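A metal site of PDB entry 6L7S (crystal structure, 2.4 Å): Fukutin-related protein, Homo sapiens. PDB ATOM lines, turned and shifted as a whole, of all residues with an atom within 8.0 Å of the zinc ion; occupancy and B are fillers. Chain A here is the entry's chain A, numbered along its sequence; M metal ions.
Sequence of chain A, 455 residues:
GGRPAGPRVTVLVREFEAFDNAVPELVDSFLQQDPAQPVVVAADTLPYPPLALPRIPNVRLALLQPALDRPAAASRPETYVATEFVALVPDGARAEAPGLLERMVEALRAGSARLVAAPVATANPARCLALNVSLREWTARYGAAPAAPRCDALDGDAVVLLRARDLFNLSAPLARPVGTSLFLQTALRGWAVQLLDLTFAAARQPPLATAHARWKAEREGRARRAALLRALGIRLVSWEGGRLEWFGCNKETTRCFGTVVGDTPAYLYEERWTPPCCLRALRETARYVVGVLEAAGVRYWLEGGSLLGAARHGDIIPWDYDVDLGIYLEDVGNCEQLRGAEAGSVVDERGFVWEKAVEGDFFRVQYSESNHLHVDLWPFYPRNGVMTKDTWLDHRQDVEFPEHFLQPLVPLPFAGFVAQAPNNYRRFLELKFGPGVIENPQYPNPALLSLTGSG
The zinc ion is bound by the side-chain sulfur (SG) of Cys 249 (2.3 Å), the side-chain sulfur (SG) of Cys 277 (2.3 Å), the side-chain sulfur (SG) of Cys 278 (2.4 Å) and the side-chain sulfur (SG) of Cys 256 (2.4 Å). The zinc ion has four donor atoms within binding distance.
ND2 of Asn 371 sits close to SG of Cys 249, 3.5 Å away. The side-chain sulfur of Cys 256 sits close to the guanidinium group of Arg 235, 3.5 Å away.
Four residues have an atom within 4 Å of the zinc ion: Cys 249, Cys 256, Cys 277 and Cys 278.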
ATOM      1  N   ARG A 235     -23.765  16.502  -1.204  1.00  0.00           N
ATOM      2  CA  ARG A 235     -22.766  17.563  -1.263  1.00  0.00           C
ATOM      3  C   ARG A 235     -22.261  17.834  -2.663  1.00  0.00           C
ATOM      4  O   ARG A 235     -21.653  18.886  -2.900  1.00  0.00           O
ATOM      5  CB  ARG A 235     -21.566  17.212  -0.365  1.00  0.00           C
ATOM      6  CG  ARG A 235     -21.874  17.106   1.124  1.00  0.00           C
ATOM      7  CD  ARG A 235     -21.792  18.456   1.829  1.00  0.00           C
ATOM      8  NE  ARG A 235     -21.796  18.290   3.276  1.00  0.00           N
ATOM      9  CZ  ARG A 235     -22.905  18.128   4.008  1.00  0.00           C
ATOM     10  NH1 ARG A 235     -24.099  18.116   3.425  1.00  0.00           N
ATOM     11  NH2 ARG A 235     -22.806  17.978   5.324  1.00  0.00           N
ATOM     12  N   TRP A 246     -21.275  21.971  -6.363  1.00  0.00           N
ATOM     13  CA  TRP A 246     -20.901  21.732  -4.973  1.00  0.00           C
ATOM     14  C   TRP A 246     -21.884  22.383  -4.010  1.00  0.00           C
ATOM     15  O   TRP A 246     -22.448  23.453  -4.279  1.00  0.00           O
ATOM     16  CB  TRP A 246     -19.486  22.254  -4.690  1.00  0.00           C
ATOM     17  CG  TRP A 246     -18.402  21.520  -5.447  1.00  0.00           C
ATOM     18  CD1 TRP A 246     -17.779  21.923  -6.594  1.00  0.00           C
ATOM     19  CD2 TRP A 246     -17.821  20.245  -5.099  1.00  0.00           C
ATOM     20  NE1 TRP A 246     -16.838  20.996  -6.970  1.00  0.00           N
ATOM     21  CE2 TRP A 246     -16.840  19.955  -6.076  1.00  0.00           C
ATOM     22  CE3 TRP A 246     -18.013  19.342  -4.056  1.00  0.00           C
ATOM     23  CZ2 TRP A 246     -16.075  18.788  -6.044  1.00  0.00           C
ATOM     24  CZ3 TRP A 246     -17.254  18.165  -4.031  1.00  0.00           C
ATOM     25  CH2 TRP A 246     -16.292  17.913  -5.022  1.00  0.00           C
ATOM     26  N   PHE A 247     -22.100  21.709  -2.878  1.00  0.00           N
ATOM     27  CA  PHE A 247     -23.056  22.123  -1.866  1.00  0.00           C
ATOM     28  C   PHE A 247     -22.514  21.883  -0.455  1.00  0.00           C
ATOM     29  O   PHE A 247     -23.285  21.592   0.468  1.00  0.00           O
ATOM     30  CB  PHE A 247     -24.399  21.408  -2.050  1.00  0.00           C
ATOM     31  CG  PHE A 247     -25.067  21.719  -3.370  1.00  0.00           C
ATOM     32  CD1 PHE A 247     -25.846  22.855  -3.515  1.00  0.00           C
ATOM     33  CD2 PHE A 247     -24.888  20.891  -4.456  1.00  0.00           C
ATOM     34  CE1 PHE A 247     -26.443  23.156  -4.724  1.00  0.00           C
ATOM     35  CE2 PHE A 247     -25.483  21.180  -5.678  1.00  0.00           C
ATOM     36  CZ  PHE A 247     -26.264  22.318  -5.809  1.00  0.00           C
ATOM     37  N   GLY A 248     -21.195  21.995  -0.281  1.00  0.00           N
ATOM     38  CA  GLY A 248     -20.556  21.689   0.984  1.00  0.00           C
ATOM     39  C   GLY A 248     -19.687  22.850   1.436  1.00  0.00           C
ATOM     40  O   GLY A 248     -20.049  24.011   1.321  1.00  0.00           O
ATOM     41  N   CYS A 249     -18.519  22.507   1.978  1.00  0.00           N
ATOM     42  CA  CYS A 249     -17.587  23.501   2.483  1.00  0.00           C
ATOM     43  C   CYS A 249     -16.668  24.012   1.364  1.00  0.00           C
ATOM     44  O   CYS A 249     -16.661  23.485   0.248  1.00  0.00           O
ATOM     45  CB  CYS A 249     -16.770  22.929   3.632  1.00  0.00           C
ATOM     46  SG  CYS A 249     -15.635  21.620   3.174  1.00  0.00           S
ATOM     47  N   ASN A 250     -15.903  25.051   1.679  1.00  0.00           N
ATOM     48  CA  ASN A 250     -14.978  25.659   0.738  1.00  0.00           C
ATOM     49  C   ASN A 250     -13.989  26.526   1.513  1.00  0.00           C
ATOM     50  O   ASN A 250     -13.948  26.499   2.738  1.00  0.00           O
ATOM     51  CB  ASN A 250     -15.725  26.467  -0.332  1.00  0.00           C
ATOM     52  CG  ASN A 250     -16.608  27.544   0.267  1.00  0.00           C
ATOM     53  OD1 ASN A 250     -16.121  28.479   0.907  1.00  0.00           O
ATOM     54  ND2 ASN A 250     -17.917  27.410   0.075  1.00  0.00           N
ATOM     55  N   THR A 253     -15.592  28.812   4.259  1.00  0.00           N
ATOM     56  CA  THR A 253     -16.443  28.261   5.291  1.00  0.00           C
ATOM     57  C   THR A 253     -15.637  27.390   6.230  1.00  0.00           C
ATOM     58  O   THR A 253     -14.451  27.118   6.030  1.00  0.00           O
ATOM     59  CB  THR A 253     -17.603  27.453   4.681  1.00  0.00           C
ATOM     60  OG1 THR A 253     -17.134  26.152   4.293  1.00  0.00           O
ATOM     61  CG2 THR A 253     -18.189  28.184   3.468  1.00  0.00           C
ATOM     62  N   THR A 254     -16.293  26.960   7.304  1.00  0.00           N
ATOM     63  CA  THR A 254     -15.746  25.913   8.141  1.00  0.00           C
ATOM     64  C   THR A 254     -15.889  24.572   7.420  1.00  0.00           C
ATOM     65  O   THR A 254     -16.698  24.411   6.500  1.00  0.00           O
ATOM     66  CB  THR A 254     -16.462  25.891   9.483  1.00  0.00           C
ATOM     67  OG1 THR A 254     -15.880  24.894  10.327  1.00  0.00           O
ATOM     68  CG2 THR A 254     -17.921  25.578   9.281  1.00  0.00           C
ATOM     69  N   ARG A 255     -15.055  23.609   7.814  1.00  0.00           N
ATOM     70  CA  ARG A 255     -15.189  22.282   7.236  1.00  0.00           C
ATOM     71  C   ARG A 255     -16.501  21.646   7.693  1.00  0.00           C
ATOM     72  O   ARG A 255     -17.087  22.033   8.712  1.00  0.00           O
ATOM     73  CB  ARG A 255     -13.984  21.407   7.576  1.00  0.00           C
ATOM     74  CG  ARG A 255     -13.930  20.875   8.995  1.00  0.00           C
ATOM     75  CD  ARG A 255     -12.614  20.152   9.263  1.00  0.00           C
ATOM     76  NE  ARG A 255     -12.444  19.809  10.679  1.00  0.00           N
ATOM     77  CZ  ARG A 255     -11.290  19.385  11.212  1.00  0.00           C
ATOM     78  NH1 ARG A 255     -10.215  19.264  10.453  1.00  0.00           N
ATOM     79  NH2 ARG A 255     -11.232  19.103  12.507  1.00  0.00           N
ATOM     80  N   CYS A 256     -16.956  20.648   6.921  1.00  0.00           N
ATOM     81  CA  CYS A 256     -18.279  20.071   7.142  1.00  0.00           C
ATOM     82  C   CYS A 256     -18.416  19.492   8.547  1.00  0.00           C
ATOM     83  O   CYS A 256     -19.390  19.787   9.253  1.00  0.00           O
ATOM     84  CB  CYS A 256     -18.536  18.984   6.095  1.00  0.00           C
ATOM     85  SG  CYS A 256     -18.764  19.647   4.434  1.00  0.00           S
ATOM     86  N   PHE A 257     -17.471  18.660   8.971  1.00  0.00           N
ATOM     87  CA  PHE A 257     -17.612  17.957  10.238  1.00  0.00           C
ATOM     88  C   PHE A 257     -17.062  18.720  11.425  1.00  0.00           C
ATOM     89  O   PHE A 257     -17.206  18.256  12.561  1.00  0.00           O
ATOM     90  CB  PHE A 257     -16.961  16.570  10.147  1.00  0.00           C
ATOM     91  CG  PHE A 257     -15.548  16.577   9.649  1.00  0.00           C
ATOM     92  CD1 PHE A 257     -15.277  16.534   8.277  1.00  0.00           C
ATOM     93  CD2 PHE A 257     -14.487  16.590  10.537  1.00  0.00           C
ATOM     94  CE1 PHE A 257     -13.971  16.527   7.823  1.00  0.00           C
ATOM     95  CE2 PHE A 257     -13.172  16.582  10.077  1.00  0.00           C
ATOM     96  CZ  PHE A 257     -12.917  16.551   8.716  1.00  0.00           C
ATOM     97  N   GLY A 258     -16.463  19.884  11.212  1.00  0.00           N
ATOM     98  CA  GLY A 258     -16.077  20.716  12.342  1.00  0.00           C
ATOM     99  C   GLY A 258     -15.065  20.048  13.246  1.00  0.00           C
ATOM    100  O   GLY A 258     -14.208  19.278  12.808  1.00  0.00           O
ATOM    101  N   THR A 274     -16.143  10.388   4.134  1.00  0.00           N
ATOM    102  CA  THR A 274     -15.747  11.786   4.123  1.00  0.00           C
ATOM    103  C   THR A 274     -16.505  12.532   3.030  1.00  0.00           C
ATOM    104  O   THR A 274     -16.605  12.037   1.904  1.00  0.00           O
ATOM    105  CB  THR A 274     -14.242  11.938   3.909  1.00  0.00           C
ATOM    106  OG1 THR A 274     -13.536  11.129   4.859  1.00  0.00           O
ATOM    107  CG2 THR A 274     -13.812  13.403   4.082  1.00  0.00           C
ATOM    108  N   PRO A 275     -17.070  13.705   3.324  1.00  0.00           N
ATOM    109  CA  PRO A 275     -17.743  14.505   2.287  1.00  0.00           C
ATOM    110  C   PRO A 275     -16.802  14.833   1.152  1.00  0.00           C
ATOM    111  O   PRO A 275     -15.608  15.081   1.362  1.00  0.00           O
ATOM    112  CB  PRO A 275     -18.169  15.769   3.049  1.00  0.00           C
ATOM    113  CG  PRO A 275     -18.319  15.311   4.456  1.00  0.00           C
ATOM    114  CD  PRO A 275     -17.249  14.266   4.673  1.00  0.00           C
ATOM    115  N   PRO A 276     -17.303  14.836  -0.095  1.00  0.00           N
ATOM    116  CA  PRO A 276     -16.404  15.044  -1.237  1.00  0.00           C
ATOM    117  C   PRO A 276     -15.831  16.444  -1.297  1.00  0.00           C
ATOM    118  O   PRO A 276     -14.725  16.624  -1.838  1.00  0.00           O
ATOM    119  CB  PRO A 276     -17.305  14.738  -2.442  1.00  0.00           C
ATOM    120  CG  PRO A 276     -18.686  15.021  -1.953  1.00  0.00           C
ATOM    121  CD  PRO A 276     -18.707  14.665  -0.489  1.00  0.00           C
ATOM    122  N   CYS A 277     -16.541  17.451  -0.777  1.00  0.00           N
ATOM    123  CA  CYS A 277     -15.974  18.795  -0.675  1.00  0.00           C
ATOM    124  C   CYS A 277     -14.784  18.811   0.266  1.00  0.00           C
ATOM    125  O   CYS A 277     -13.791  19.511   0.012  1.00  0.00           O
ATOM    126  CB  CYS A 277     -17.045  19.776  -0.176  1.00  0.00           C
ATOM    127  SG  CYS A 277     -17.922  19.145   1.275  1.00  0.00           S
ATOM    128  N   CYS A 278     -14.862  18.052   1.374  1.00  0.00           N
ATOM    129  CA  CYS A 278     -13.735  17.956   2.295  1.00  0.00           C
ATOM    130  C   CYS A 278     -12.559  17.221   1.658  1.00  0.00           C
ATOM    131  O   CYS A 278     -11.399  17.589   1.859  1.00  0.00           O
ATOM    132  CB  CYS A 278     -14.169  17.259   3.574  1.00  0.00           C
ATOM    133  SG  CYS A 278     -15.427  18.089   4.570  1.00  0.00           S
ATOM    134  N   LEU A 279     -12.843  16.170   0.884  1.00  0.00           N
ATOM    135  CA  LEU A 279     -11.780  15.461   0.180  1.00  0.00           C
ATOM    136  C   LEU A 279     -11.163  16.333  -0.898  1.00  0.00           C
ATOM    137  O   LEU A 279      -9.944  16.300  -1.117  1.00  0.00           O
ATOM    138  CB  LEU A 279     -12.309  14.159  -0.422  1.00  0.00           C
ATOM    139  CG  LEU A 279     -12.610  13.032   0.571  1.00  0.00           C
ATOM    140  CD1 LEU A 279     -13.237  11.831  -0.155  1.00  0.00           C
ATOM    141  CD2 LEU A 279     -11.352  12.639   1.351  1.00  0.00           C
ATOM    142  N   ARG A 280     -11.992  17.106  -1.609  1.00  0.00           N
ATOM    143  CA  ARG A 280     -11.473  17.983  -2.650  1.00  0.00           C
ATOM    144  C   ARG A 280     -10.517  19.026  -2.054  1.00  0.00           C
ATOM    145  O   ARG A 280      -9.437  19.254  -2.616  1.00  0.00           O
ATOM    146  CB  ARG A 280     -12.637  18.661  -3.374  1.00  0.00           C
ATOM    147  CG  ARG A 280     -12.246  19.430  -4.636  1.00  0.00           C
ATOM    148  CD  ARG A 280     -13.136  20.647  -4.804  1.00  0.00           C
ATOM    149  NE  ARG A 280     -13.077  21.519  -3.626  1.00  0.00           N
ATOM    150  CZ  ARG A 280     -12.112  22.388  -3.377  1.00  0.00           C
ATOM    151  NH1 ARG A 280     -11.101  22.540  -4.235  1.00  0.00           N
ATOM    152  NH2 ARG A 280     -12.150  23.124  -2.278  1.00  0.00           N
ATOM    153  N   ALA A 281     -10.881  19.631  -0.920  1.00  0.00           N
ATOM    154  CA  ALA A 281      -9.994  20.587  -0.288  1.00  0.00           C
ATOM    155  C   ALA A 281      -8.717  19.927   0.220  1.00  0.00           C
ATOM    156  O   ALA A 281      -7.646  20.557   0.191  1.00  0.00           O
ATOM    157  CB  ALA A 281     -10.708  21.310   0.854  1.00  0.00           C
ATOM    158  N   ASN A 371     -11.392  27.072   7.239  1.00  0.00           N
ATOM    159  CA  ASN A 371     -11.523  25.647   6.908  1.00  0.00           C
ATOM    160  C   ASN A 371     -10.269  24.904   7.378  1.00  0.00           C
ATOM    161  O   ASN A 371      -9.178  25.104   6.833  1.00  0.00           O
ATOM    162  CB  ASN A 371     -11.721  25.460   5.403  1.00  0.00           C
ATOM    163  CG  ASN A 371     -12.241  24.062   5.055  1.00  0.00           C
ATOM    164  OD1 ASN A 371     -11.802  23.062   5.630  1.00  0.00           O
ATOM    165  ND2 ASN A 371     -13.166  23.990   4.104  1.00  0.00           N
ATOM    166  N   LEU A 373      -9.358  21.643   7.385  1.00  0.00           N
ATOM    167  CA  LEU A 373      -8.789  20.476   6.733  1.00  0.00           C
ATOM    168  C   LEU A 373      -7.293  20.691   6.533  1.00  0.00           C
ATOM    169  O   LEU A 373      -6.874  21.753   6.049  1.00  0.00           O
ATOM    170  CB  LEU A 373      -9.489  20.215   5.407  1.00  0.00           C
ATOM    171  CG  LEU A 373     -10.971  19.844   5.544  1.00  0.00           C
ATOM    172  CD1 LEU A 373     -11.721  20.110   4.254  1.00  0.00           C
ATOM    173  CD2 LEU A 373     -11.139  18.382   5.992  1.00  0.00           C
HETATM  174 ZN    ZN M   1     -16.722  19.548   3.253  1.00  0.00          ZN
